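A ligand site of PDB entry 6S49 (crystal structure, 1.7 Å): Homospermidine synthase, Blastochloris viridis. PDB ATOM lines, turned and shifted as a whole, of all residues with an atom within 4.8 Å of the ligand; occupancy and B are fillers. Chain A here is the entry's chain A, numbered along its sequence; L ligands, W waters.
Water W6 lies within hydrogen-bond range of O5 of the ligand, OG of Ser 50 and NH2 of Arg 27. Water W5 lies within hydrogen-bond range of an oxygen (O8) of the ligand (2.7 Å), the backbone carbonyl oxygen of Leu 94 (2.8 Å), the backbone NH of Gly 26 (2.9 Å) and the backbone NH of Gly 23 (2.9 Å). Water W1 bridges OD2 of Asp 97 (2.7 Å) and N2 of the ligand (2.8 Å). Water W2 lies within hydrogen-bond range of O2 of the ligand (2.9 Å), N of Val 234 (3.0 Å) and OG of Ser 233 (3.4 Å).
The backbone carbonyl oxygen (O) of Val 96 sits close to a nitrogen (N2) of the ligand (3.3 Å). A nitrogen (N7) of the ligand sits close to the backbone NH (N) of Ala 164, at 2.9 Å. The backbone carbonyl oxygen of Pro 166 lies close to an oxygen (O14) of the ligand, at 3.2 Å. Merely in contact with the ligand: Val 118, Gly 23, Pro 49, Ile 353, Leu 94, Trp 232, Ala 68, Val 403, Thr 98, Gly 163, Phe 22, Ser 50, Ile 20 and Asp 97. Of the 34 residues printed, 25 come within 4 Å of the ligand. The nearest printed residue that does not touch the ligand is Gly 21 (4.04 Å).
OD2 of Asp 48 lies within hydrogen-bond range of N of Phe 22, at 2.7 Å. The side-chain carboxylate (OD1) of Asp 48 lies within hydrogen-bond range of the backbone NH (N) of Ser 50, at 3.0 Å. OG of Ser 95 lies within hydrogen-bond range of OG1 of Thr 98, at 2.6 Å. N of Ser 95 lies within hydrogen-bond range of O of Ile 20, 3.4 Å away. The backbone NH (N) of Gly 236 sits at hydrogen-bond distance from the side-chain hydroxyl (OG) of Ser 233, 2.8 Å away. The backbone carbonyl oxygen (O) of Gly 23 sits close to the guanidinium group (NE) of Arg 27 (3.3 Å). The backbone carbonyl oxygen (O) of Ile 20 is in hydrogen-bond range of the backbone NH (N) of Leu 94 (2.8 Å). N of Asp 97 is in hydrogen-bond range of OE2 of Glu 120, 2.9 Å away.
The side-chain carboxylate of Asp 48 sits at hydrogen-bond distance from an oxygen (O6) of the ligand (2.7 Å). The backbone NH of Ser 24 is in hydrogen-bond range of an oxygen (O1) of the ligand, 3.1 Å away. An oxygen (O9) of the ligand sits at hydrogen-bond distance from the side-chain hydroxyl (OG) of Ser 24 (2.7 Å). The backbone carbonyl oxygen (O) of Ser 95 is in hydrogen-bond range of an oxygen (O12) of the ligand (2.8 Å). N of Val 69 sits at hydrogen-bond distance from N4 of the ligand (3.2 Å). O of Val 69 sits at hydrogen-bond distance from N3 of the ligand, at 2.9 Å. N of Ile 25 is in hydrogen-bond range of O8 of the ligand, 2.9 Å away. The backbone carbonyl oxygen (O) of Asn 165 lies within hydrogen-bond range of a nitrogen (N7) of the ligand (3.2 Å). An oxygen (O9) of the ligand is in hydrogen-bond range of the backbone NH (N) of Ser 233, 3.0 Å away. The side-chain hydroxyl (OG) of Ser 233 is in hydrogen-bond range of an oxygen (O2) of the ligand (2.9 Å). OG1 of Thr 117 sits close to O11 of the ligand, 3.0 Å away.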
ATOM      1  N   ILE A  20      24.149  -5.043 -16.693  1.00  0.00           N
ATOM      2  CA  ILE A  20      22.910  -4.357 -16.420  1.00  0.00           C
ATOM      3  C   ILE A  20      23.215  -3.341 -15.341  1.00  0.00           C
ATOM      4  O   ILE A  20      23.569  -3.706 -14.204  1.00  0.00           O
ATOM      5  CB  ILE A  20      21.800  -5.321 -15.970  1.00  0.00           C
ATOM      6  CG1 ILE A  20      21.600  -6.423 -17.017  1.00  0.00           C
ATOM      7  CG2 ILE A  20      20.495  -4.573 -15.739  1.00  0.00           C
ATOM      8  CD1 ILE A  20      20.611  -7.484 -16.581  1.00  0.00           C
ATOM      9  N   GLY A  21      23.088  -2.069 -15.690  1.00  0.00           N
ATOM     10  CA  GLY A  21      23.472  -1.011 -14.787  1.00  0.00           C
ATOM     11  C   GLY A  21      24.884  -0.519 -15.023  1.00  0.00           C
ATOM     12  O   GLY A  21      25.825  -1.312 -15.076  1.00  0.00           O
ATOM     13  N   PHE A  22      25.042   0.792 -15.123  1.00  0.00           N
ATOM     14  CA  PHE A  22      26.340   1.388 -15.333  1.00  0.00           C
ATOM     15  C   PHE A  22      26.430   2.665 -14.501  1.00  0.00           C
ATOM     16  O   PHE A  22      26.620   3.770 -14.994  1.00  0.00           O
ATOM     17  CB  PHE A  22      26.544   1.622 -16.833  1.00  0.00           C
ATOM     18  CG  PHE A  22      27.992   1.795 -17.220  1.00  0.00           C
ATOM     19  CD1 PHE A  22      28.895   0.772 -17.052  1.00  0.00           C
ATOM     20  CD2 PHE A  22      28.453   3.010 -17.746  1.00  0.00           C
ATOM     21  CE1 PHE A  22      30.226   0.916 -17.411  1.00  0.00           C
ATOM     22  CE2 PHE A  22      29.790   3.168 -18.099  1.00  0.00           C
ATOM     23  CZ  PHE A  22      30.675   2.114 -17.922  1.00  0.00           C
ATOM     24  N   GLY A  23      26.274   2.493 -13.199  1.00  0.00           N
ATOM     25  CA  GLY A  23      26.536   3.544 -12.222  1.00  0.00           C
ATOM     26  C   GLY A  23      27.913   3.395 -11.625  1.00  0.00           C
ATOM     27  O   GLY A  23      28.857   2.997 -12.303  1.00  0.00           O
ATOM     28  N   SER A  24      28.042   3.717 -10.333  1.00  0.00           N
ATOM     29  CA  SER A  24      29.378   3.787  -9.760  1.00  0.00           C
ATOM     30  C   SER A  24      30.072   2.419  -9.798  1.00  0.00           C
ATOM     31  O   SER A  24      31.276   2.339 -10.087  1.00  0.00           O
ATOM     32  CB  SER A  24      29.323   4.350  -8.334  1.00  0.00           C
ATOM     33  OG  SER A  24      29.178   3.352  -7.340  1.00  0.00           O
ATOM     34  N   ILE A  25      29.342   1.329  -9.557  1.00  0.00           N
ATOM     35  CA  ILE A  25      29.990   0.029  -9.515  1.00  0.00           C
ATOM     36  C   ILE A  25      30.197  -0.523 -10.926  1.00  0.00           C
ATOM     37  O   ILE A  25      31.248  -1.085 -11.232  1.00  0.00           O
ATOM     38  CB  ILE A  25      29.182  -0.950  -8.633  1.00  0.00           C
ATOM     39  CG1 ILE A  25      29.053  -0.399  -7.194  1.00  0.00           C
ATOM     40  CG2 ILE A  25      29.802  -2.330  -8.658  1.00  0.00           C
ATOM     41  CD1 ILE A  25      30.369   0.053  -6.551  1.00  0.00           C
ATOM     42  N   GLY A  26      29.214  -0.375 -11.820  1.00  0.00           N
ATOM     43  CA  GLY A  26      29.421  -0.775 -13.197  1.00  0.00           C
ATOM     44  C   GLY A  26      30.634  -0.084 -13.808  1.00  0.00           C
ATOM     45  O   GLY A  26      31.434  -0.711 -14.513  1.00  0.00           O
ATOM     46  N   ARG A  27      30.791   1.213 -13.530  1.00  0.00           N
ATOM     47  CA  ARG A  27      31.925   1.956 -14.089  1.00  0.00           C
ATOM     48  C   ARG A  27      33.256   1.463 -13.546  1.00  0.00           C
ATOM     49  O   ARG A  27      34.267   1.467 -14.259  1.00  0.00           O
ATOM     50  CB  ARG A  27      31.758   3.449 -13.789  1.00  0.00           C
ATOM     51  CG  ARG A  27      30.608   4.052 -14.549  1.00  0.00           C
ATOM     52  CD  ARG A  27      30.040   5.329 -13.911  1.00  0.00           C
ATOM     53  NE  ARG A  27      28.665   5.521 -14.353  1.00  0.00           N
ATOM     54  CZ  ARG A  27      27.947   6.635 -14.171  1.00  0.00           C
ATOM     55  NH1 ARG A  27      28.484   7.677 -13.553  1.00  0.00           N
ATOM     56  NH2 ARG A  27      26.686   6.692 -14.612  1.00  0.00           N
ATOM     57  N   ILE A  47      23.455  -2.011 -20.442  1.00  0.00           N
ATOM     58  CA  ILE A  47      22.060  -1.588 -20.441  1.00  0.00           C
ATOM     59  C   ILE A  47      21.861  -0.658 -19.262  1.00  0.00           C
ATOM     60  O   ILE A  47      22.109  -1.045 -18.107  1.00  0.00           O
ATOM     61  CB  ILE A  47      21.097  -2.785 -20.351  1.00  0.00           C
ATOM     62  CG1 ILE A  47      21.437  -3.848 -21.394  1.00  0.00           C
ATOM     63  CG2 ILE A  47      19.664  -2.281 -20.518  1.00  0.00           C
ATOM     64  CD1 ILE A  47      20.765  -5.158 -21.110  1.00  0.00           C
ATOM     65  N   ASP A  48      21.389   0.554 -19.535  1.00  0.00           N
ATOM     66  CA  ASP A  48      21.127   1.515 -18.463  1.00  0.00           C
ATOM     67  C   ASP A  48      20.233   2.616 -19.014  1.00  0.00           C
ATOM     68  O   ASP A  48      20.446   3.045 -20.147  1.00  0.00           O
ATOM     69  CB  ASP A  48      22.431   2.127 -17.946  1.00  0.00           C
ATOM     70  CG  ASP A  48      22.266   2.860 -16.651  1.00  0.00           C
ATOM     71  OD1 ASP A  48      21.514   3.859 -16.602  1.00  0.00           O
ATOM     72  OD2 ASP A  48      22.938   2.453 -15.681  1.00  0.00           O
ATOM     73  N   PRO A  49      19.244   3.084 -18.257  1.00  0.00           N
ATOM     74  CA  PRO A  49      18.310   4.081 -18.808  1.00  0.00           C
ATOM     75  C   PRO A  49      18.858   5.509 -18.878  1.00  0.00           C
ATOM     76  O   PRO A  49      18.227   6.337 -19.553  1.00  0.00           O
ATOM     77  CB  PRO A  49      17.113   4.012 -17.854  1.00  0.00           C
ATOM     78  CG  PRO A  49      17.687   3.528 -16.569  1.00  0.00           C
ATOM     79  CD  PRO A  49      18.747   2.531 -16.984  1.00  0.00           C
ATOM     80  N   SER A  50      19.973   5.821 -18.232  1.00  0.00           N
ATOM     81  CA  SER A  50      20.389   7.214 -18.056  1.00  0.00           C
ATOM     82  C   SER A  50      21.282   7.709 -19.180  1.00  0.00           C
ATOM     83  O   SER A  50      22.133   6.967 -19.697  1.00  0.00           O
ATOM     84  CB  SER A  50      21.105   7.371 -16.727  1.00  0.00           C
ATOM     85  OG  SER A  50      22.473   7.105 -16.881  1.00  0.00           O
ATOM     86  N   ALA A  53      25.006   7.507 -18.130  1.00  0.00           N
ATOM     87  CA  ALA A  53      25.626   6.220 -18.395  1.00  0.00           C
ATOM     88  C   ALA A  53      25.928   6.036 -19.873  1.00  0.00           C
ATOM     89  O   ALA A  53      26.977   5.518 -20.247  1.00  0.00           O
ATOM     90  CB  ALA A  53      24.728   5.083 -17.880  1.00  0.00           C
ATOM     91  N   GLN A  67      17.843   1.600 -21.937  1.00  0.00           N
ATOM     92  CA  GLN A  67      16.539   1.110 -21.512  1.00  0.00           C
ATOM     93  C   GLN A  67      16.600   0.801 -20.032  1.00  0.00           C
ATOM     94  O   GLN A  67      17.628   0.369 -19.512  1.00  0.00           O
ATOM     95  CB  GLN A  67      16.097  -0.164 -22.253  1.00  0.00           C
ATOM     96  CG  GLN A  67      15.764   0.008 -23.711  1.00  0.00           C
ATOM     97  CD  GLN A  67      14.473   0.762 -23.942  1.00  0.00           C
ATOM     98  OE1 GLN A  67      13.618   0.849 -23.052  1.00  0.00           O
ATOM     99  NE2 GLN A  67      14.311   1.300 -25.148  1.00  0.00           N
ATOM    100  N   ALA A  68      15.490   1.049 -19.356  1.00  0.00           N
ATOM    101  CA  ALA A  68      15.263   0.474 -18.043  1.00  0.00           C
ATOM    102  C   ALA A  68      14.751  -0.949 -18.194  1.00  0.00           C
ATOM    103  O   ALA A  68      13.784  -1.203 -18.930  1.00  0.00           O
ATOM    104  CB  ALA A  68      14.266   1.316 -17.254  1.00  0.00           C
ATOM    105  N   VAL A  69      15.424  -1.896 -17.541  1.00  0.00           N
ATOM    106  CA  VAL A  69      14.921  -3.264 -17.447  1.00  0.00           C
ATOM    107  C   VAL A  69      13.755  -3.271 -16.464  1.00  0.00           C
ATOM    108  O   VAL A  69      13.902  -2.793 -15.332  1.00  0.00           O
ATOM    109  CB  VAL A  69      16.032  -4.219 -17.002  1.00  0.00           C
ATOM    110  CG1 VAL A  69      15.508  -5.665 -16.927  1.00  0.00           C
ATOM    111  CG2 VAL A  69      17.259  -4.101 -17.910  1.00  0.00           C
ATOM    112  N   LEU A  94      24.474  -4.982 -11.940  1.00  0.00           N
ATOM    113  CA  LEU A  94      24.935  -3.930 -11.041  1.00  0.00           C
ATOM    114  C   LEU A  94      23.961  -2.775 -11.088  1.00  0.00           C
ATOM    115  O   LEU A  94      24.347  -1.611 -11.164  1.00  0.00           O
ATOM    116  CB  LEU A  94      26.351  -3.521 -11.423  1.00  0.00           C
ATOM    117  CG  LEU A  94      27.362  -4.662 -11.532  1.00  0.00           C
ATOM    118  CD1 LEU A  94      28.681  -4.163 -12.143  1.00  0.00           C
ATOM    119  CD2 LEU A  94      27.584  -5.317 -10.169  1.00  0.00           C
ATOM    120  N   SER A  95      22.674  -3.091 -10.993  1.00  0.00           N
ATOM    121  CA  SER A  95      21.606  -2.119 -11.210  1.00  0.00           C
ATOM    122  C   SER A  95      20.829  -1.867  -9.914  1.00  0.00           C
ATOM    123  O   SER A  95      21.032  -2.522  -8.884  1.00  0.00           O
ATOM    124  CB  SER A  95      20.660  -2.625 -12.297  1.00  0.00           C
ATOM    125  OG  SER A  95      20.029  -3.833 -11.929  1.00  0.00           O
ATOM    126  N   VAL A  96      19.955  -0.864  -9.970  1.00  0.00           N
ATOM    127  CA  VAL A  96      18.888  -0.703  -8.982  1.00  0.00           C
ATOM    128  C   VAL A  96      17.551  -0.918  -9.709  1.00  0.00           C
ATOM    129  O   VAL A  96      17.470  -0.866 -10.937  1.00  0.00           O
ATOM    130  CB  VAL A  96      18.897   0.669  -8.282  1.00  0.00           C
ATOM    131  CG1 VAL A  96      20.186   0.847  -7.463  1.00  0.00           C
ATOM    132  CG2 VAL A  96      18.753   1.790  -9.288  1.00  0.00           C
ATOM    133  N   ASP A  97      16.499  -1.159  -8.923  1.00  0.00           N
ATOM    134  CA  ASP A  97      15.115  -1.166  -9.403  1.00  0.00           C
ATOM    135  C   ASP A  97      14.768  -2.394 -10.225  1.00  0.00           C
ATOM    136  O   ASP A  97      13.676  -2.435 -10.826  1.00  0.00           O
ATOM    137  CB  ASP A  97      14.802   0.104 -10.215  1.00  0.00           C
ATOM    138  CG  ASP A  97      14.902   1.383  -9.380  1.00  0.00           C
ATOM    139  OD1 ASP A  97      15.013   1.274  -8.138  1.00  0.00           O
ATOM    140  OD2 ASP A  97      14.848   2.494  -9.953  1.00  0.00           O
ATOM    141  N   THR A  98      15.624  -3.407 -10.253  1.00  0.00           N
ATOM    142  CA  THR A  98      15.430  -4.627 -11.021  1.00  0.00           C
ATOM    143  C   THR A  98      15.378  -5.834 -10.082  1.00  0.00           C
ATOM    144  O   THR A  98      15.998  -5.839  -9.016  1.00  0.00           O
ATOM    145  CB  THR A  98      16.569  -4.818 -12.015  1.00  0.00           C
ATOM    146  OG1 THR A  98      17.805  -4.914 -11.286  1.00  0.00           O
ATOM    147  CG2 THR A  98      16.645  -3.658 -13.006  1.00  0.00           C
ATOM    148  N   THR A 117      25.113  -8.022  -6.603  1.00  0.00           N
ATOM    149  CA  THR A 117      25.662  -7.564  -5.337  1.00  0.00           C
ATOM    150  C   THR A 117      24.572  -7.242  -4.316  1.00  0.00           C
ATOM    151  O   THR A 117      24.885  -6.655  -3.266  1.00  0.00           O
ATOM    152  CB  THR A 117      26.529  -6.315  -5.509  1.00  0.00           C
ATOM    153  OG1 THR A 117      25.736  -5.183  -5.862  1.00  0.00           O
ATOM    154  CG2 THR A 117      27.615  -6.537  -6.555  1.00  0.00           C
ATOM    155  N   VAL A 118      23.329  -7.614  -4.586  1.00  0.00           N
ATOM    156  CA  VAL A 118      22.182  -7.266  -3.773  1.00  0.00           C
ATOM    157  C   VAL A 118      21.033  -8.115  -4.275  1.00  0.00           C
ATOM    158  O   VAL A 118      20.977  -8.396  -5.478  1.00  0.00           O
ATOM    159  CB  VAL A 118      21.871  -5.765  -3.855  1.00  0.00           C
ATOM    160  CG1 VAL A 118      21.612  -5.330  -5.292  1.00  0.00           C
ATOM    161  CG2 VAL A 118      20.683  -5.403  -2.982  1.00  0.00           C
ATOM    162  N   GLU A 120      17.895  -7.334  -5.148  1.00  0.00           N
ATOM    163  CA  GLU A 120      17.070  -6.177  -5.443  1.00  0.00           C
ATOM    164  C   GLU A 120      15.708  -6.633  -5.950  1.00  0.00           C
ATOM    165  O   GLU A 120      15.595  -7.687  -6.604  1.00  0.00           O
ATOM    166  CB  GLU A 120      17.765  -5.303  -6.492  1.00  0.00           C
ATOM    167  CG  GLU A 120      17.059  -4.011  -6.830  1.00  0.00           C
ATOM    168  CD  GLU A 120      17.325  -2.899  -5.844  1.00  0.00           C
ATOM    169  OE1 GLU A 120      17.861  -3.170  -4.755  1.00  0.00           O
ATOM    170  OE2 GLU A 120      16.994  -1.736  -6.171  1.00  0.00           O
ATOM    171  N   GLY A 163      29.396  -8.534  -3.715  1.00  0.00           N
ATOM    172  CA  GLY A 163      30.108  -7.275  -3.705  1.00  0.00           C
ATOM    173  C   GLY A 163      31.131  -7.260  -2.582  1.00  0.00           C
ATOM    174  O   GLY A 163      31.702  -8.297  -2.226  1.00  0.00           O
ATOM    175  N   ALA A 164      31.340  -6.075  -2.000  1.00  0.00           N
ATOM    176  CA  ALA A 164      32.227  -5.957  -0.847  1.00  0.00           C
ATOM    177  C   ALA A 164      31.528  -6.444   0.415  1.00  0.00           C
ATOM    178  O   ALA A 164      32.098  -7.215   1.192  1.00  0.00           O
ATOM    179  CB  ALA A 164      32.666  -4.494  -0.694  1.00  0.00           C
ATOM    180  N   ASN A 165      30.337  -5.954   0.669  1.00  0.00           N
ATOM    181  CA  ASN A 165      29.505  -6.381   1.784  1.00  0.00           C
ATOM    182  C   ASN A 165      28.052  -6.131   1.426  1.00  0.00           C
ATOM    183  O   ASN A 165      27.623  -4.971   1.356  1.00  0.00           O
ATOM    184  CB  ASN A 165      29.890  -5.651   3.084  1.00  0.00           C
ATOM    185  CG  ASN A 165      29.964  -4.131   2.926  1.00  0.00           C
ATOM    186  OD1 ASN A 165      30.194  -3.597   1.842  1.00  0.00           O
ATOM    187  ND2 ASN A 165      29.808  -3.440   4.023  1.00  0.00           N
ATOM    188  N   PRO A 166      27.248  -7.176   1.143  1.00  0.00           N
ATOM    189  CA  PRO A 166      27.611  -8.598   1.126  1.00  0.00           C
ATOM    190  C   PRO A 166      28.627  -8.937   0.039  1.00  0.00           C
ATOM    191  O   PRO A 166      28.727  -8.242  -0.969  1.00  0.00           O
ATOM    192  CB  PRO A 166      26.284  -9.295   0.849  1.00  0.00           C
ATOM    193  CG  PRO A 166      25.478  -8.282   0.081  1.00  0.00           C
ATOM    194  CD  PRO A 166      25.845  -6.961   0.750  1.00  0.00           C
ATOM    195  N   TRP A 232      29.007   5.709  -2.841  1.00  0.00           N
ATOM    196  CA  TRP A 232      28.391   4.702  -3.712  1.00  0.00           C
ATOM    197  C   TRP A 232      26.911   5.041  -3.796  1.00  0.00           C
ATOM    198  O   TRP A 232      26.466   6.037  -3.226  1.00  0.00           O
ATOM    199  CB  TRP A 232      28.646   3.300  -3.174  1.00  0.00           C
ATOM    200  CG  TRP A 232      28.031   3.052  -1.830  1.00  0.00           C
ATOM    201  CD1 TRP A 232      28.512   3.463  -0.625  1.00  0.00           C
ATOM    202  CD2 TRP A 232      26.829   2.322  -1.546  1.00  0.00           C
ATOM    203  NE1 TRP A 232      27.693   3.060   0.379  1.00  0.00           N
ATOM    204  CE2 TRP A 232      26.649   2.348  -0.159  1.00  0.00           C
ATOM    205  CE3 TRP A 232      25.883   1.660  -2.339  1.00  0.00           C
ATOM    206  CZ2 TRP A 232      25.569   1.718   0.460  1.00  0.00           C
ATOM    207  CZ3 TRP A 232      24.824   1.039  -1.728  1.00  0.00           C
ATOM    208  CH2 TRP A 232      24.659   1.092  -0.337  1.00  0.00           C
ATOM    209  N   SER A 233      26.124   4.209  -4.487  1.00  0.00           N
ATOM    210  CA  SER A 233      24.718   4.475  -4.754  1.00  0.00           C
ATOM    211  C   SER A 233      24.021   5.241  -3.633  1.00  0.00           C
ATOM    212  O   SER A 233      23.901   4.746  -2.516  1.00  0.00           O
ATOM    213  CB  SER A 233      23.938   3.181  -4.958  1.00  0.00           C
ATOM    214  OG  SER A 233      22.666   3.472  -5.513  1.00  0.00           O
ATOM    215  N   VAL A 234      23.530   6.434  -3.940  1.00  0.00           N
ATOM    216  CA  VAL A 234      22.628   7.102  -3.000  1.00  0.00           C
ATOM    217  C   VAL A 234      21.276   6.413  -2.988  1.00  0.00           C
ATOM    218  O   VAL A 234      20.733   6.122  -1.923  1.00  0.00           O
ATOM    219  CB  VAL A 234      22.513   8.592  -3.342  1.00  0.00           C
ATOM    220  CG1 VAL A 234      21.388   9.237  -2.543  1.00  0.00           C
ATOM    221  CG2 VAL A 234      23.853   9.287  -3.071  1.00  0.00           C
ATOM    222  N   GLY A 236      20.529   3.361  -3.686  1.00  0.00           N
ATOM    223  CA  GLY A 236      20.651   2.055  -3.044  1.00  0.00           C
ATOM    224  C   GLY A 236      20.860   2.159  -1.551  1.00  0.00           C
ATOM    225  O   GLY A 236      20.315   1.364  -0.775  1.00  0.00           O
ATOM    226  N   ILE A 353      27.231  11.178  -5.938  1.00  0.00           N
ATOM    227  CA  ILE A 353      28.218  10.182  -5.553  1.00  0.00           C
ATOM    228  C   ILE A 353      29.601  10.759  -5.793  1.00  0.00           C
ATOM    229  O   ILE A 353      29.916  11.192  -6.914  1.00  0.00           O
ATOM    230  CB  ILE A 353      28.030   8.870  -6.347  1.00  0.00           C
ATOM    231  CG1 ILE A 353      26.626   8.306  -6.121  1.00  0.00           C
ATOM    232  CG2 ILE A 353      29.135   7.872  -5.965  1.00  0.00           C
ATOM    233  CD1 ILE A 353      26.297   7.141  -7.023  1.00  0.00           C
ATOM    234  N   VAL A 403      34.207  -3.212  -4.065  1.00  0.00           N
ATOM    235  CA  VAL A 403      33.032  -3.880  -4.625  1.00  0.00           C
ATOM    236  C   VAL A 403      33.355  -4.501  -5.973  1.00  0.00           C
ATOM    237  O   VAL A 403      33.079  -5.682  -6.220  1.00  0.00           O
ATOM    238  CB  VAL A 403      31.852  -2.894  -4.750  1.00  0.00           C
ATOM    239  CG1 VAL A 403      30.632  -3.590  -5.314  1.00  0.00           C
ATOM    240  CG2 VAL A 403      31.543  -2.237  -3.402  1.00  0.00           C
HETATM  241  P1  LIG L   1      24.290   3.734  -8.784  1.00  0.00           P
HETATM  242  O1  LIG L   1      25.380   4.418  -8.961  1.00  0.00           O
HETATM  243  O2  LIG L   1      23.210   4.390  -8.242  1.00  0.00           O
HETATM  244  O3  LIG L   1      23.874   3.212 -10.181  1.00  0.00           O
HETATM  245  C1  LIG L   1      22.764   2.481 -10.409  1.00  0.00           C
HETATM  246  C2  LIG L   1      22.455   2.401 -11.904  1.00  0.00           C
HETATM  247  O4  LIG L   1      21.312   1.663 -12.163  1.00  0.00           O
HETATM  248  C3  LIG L   1      22.199   3.783 -12.502  1.00  0.00           C
HETATM  249  O5  LIG L   1      23.114   4.138 -13.507  1.00  0.00           O
HETATM  250  C4  LIG L   1      20.765   3.687 -13.040  1.00  0.00           C
HETATM  251  O6  LIG L   1      20.457   4.446 -14.159  1.00  0.00           O
HETATM  252  C5  LIG L   1      20.622   2.193 -13.244  1.00  0.00           C
HETATM  253  N1  LIG L   1      19.250   1.787 -13.313  1.00  0.00           N
HETATM  254  C6  LIG L   1      18.159   2.294 -12.728  1.00  0.00           C
HETATM  255  N2  LIG L   1      17.084   1.610 -13.093  1.00  0.00           N
HETATM  256  C7  LIG L   1      17.466   0.651 -13.936  1.00  0.00           C
HETATM  257  C8  LIG L   1      16.796  -0.416 -14.672  1.00  0.00           C
HETATM  258  N3  LIG L   1      15.479  -0.555 -14.531  1.00  0.00           N
HETATM  259  N4  LIG L   1      17.614  -1.159 -15.386  1.00  0.00           N
HETATM  260  C9  LIG L   1      18.907  -0.965 -15.480  1.00  0.00           C
HETATM  261  N5  LIG L   1      19.557  -0.027 -14.843  1.00  0.00           N
HETATM  262  C10 LIG L   1      18.914   0.760 -14.027  1.00  0.00           C
HETATM  263  O7  LIG L   1      24.553   2.440  -7.922  1.00  0.00           O
HETATM  264  P2  LIG L   1      25.907   1.690  -7.693  1.00  0.00           P
HETATM  265  O8  LIG L   1      26.514   1.357  -8.919  1.00  0.00           O
HETATM  266  O9  LIG L   1      26.698   2.316  -6.765  1.00  0.00           O
HETATM  267  O10 LIG L   1      25.302   0.418  -7.053  1.00  0.00           O
HETATM  268  C11 LIG L   1      24.706  -0.520  -7.857  1.00  0.00           C
HETATM  269  C12 LIG L   1      24.066  -1.735  -7.210  1.00  0.00           C
HETATM  270  O11 LIG L   1      25.008  -2.365  -6.397  1.00  0.00           O
HETATM  271  C13 LIG L   1      22.964  -1.263  -6.311  1.00  0.00           C
HETATM  272  O12 LIG L   1      21.845  -2.115  -6.242  1.00  0.00           O
HETATM  273  C14 LIG L   1      23.688  -1.246  -4.973  1.00  0.00           C
HETATM  274  O13 LIG L   1      22.874  -1.357  -3.835  1.00  0.00           O
HETATM  275  C15 LIG L   1      24.624  -2.444  -5.071  1.00  0.00           C
HETATM  276  N6  LIG L   1      25.845  -2.362  -4.232  1.00  0.00           N
HETATM  277  C16 LIG L   1      26.271  -3.386  -3.575  1.00  0.00           C
HETATM  278  C17 LIG L   1      27.391  -3.341  -2.768  1.00  0.00           C
HETATM  279  C18 LIG L   1      27.938  -4.529  -1.990  1.00  0.00           C
HETATM  280  O14 LIG L   1      27.287  -5.568  -1.976  1.00  0.00           O
HETATM  281  N7  LIG L   1      29.078  -4.400  -1.447  1.00  0.00           N
HETATM  282  C19 LIG L   1      28.076  -2.143  -2.762  1.00  0.00           C
HETATM  283  C20 LIG L   1      27.660  -1.110  -3.582  1.00  0.00           C
HETATM  284  C21 LIG L   1      26.527  -1.258  -4.300  1.00  0.00           C
HETATM  285  O   HOH W   1      14.524   2.504 -12.634  1.00  0.00           O
HETATM  286  O   HOH W   2      22.420   6.661  -6.672  1.00  0.00           O
HETATM  287  O   HOH W   3      28.978  -0.183  -0.486  1.00  0.00           O
HETATM  288  O   HOH W   4      26.041   6.736 -10.660  1.00  0.00           O
HETATM  289  O   HOH W   5      26.417   0.229 -11.382  1.00  0.00           O
HETATM  290  O   HOH W   6      23.630   6.647 -14.372  1.00  0.00           O
HETATM  291  O   HOH W   7      17.078   4.545 -10.675  1.00  0.00           O
HETATM  292  O   HOH W   8      26.818  -2.362   0.484  1.00  0.00           O
HETATM  293  O   HOH W   9      12.687   0.926 -13.930  1.00  0.00           O
HETATM  294  O   HOH W  10      20.843   5.268  -9.599  1.00  0.00           O
HETATM  295  O   HOH W  11      18.847   6.510 -13.641  1.00  0.00           O
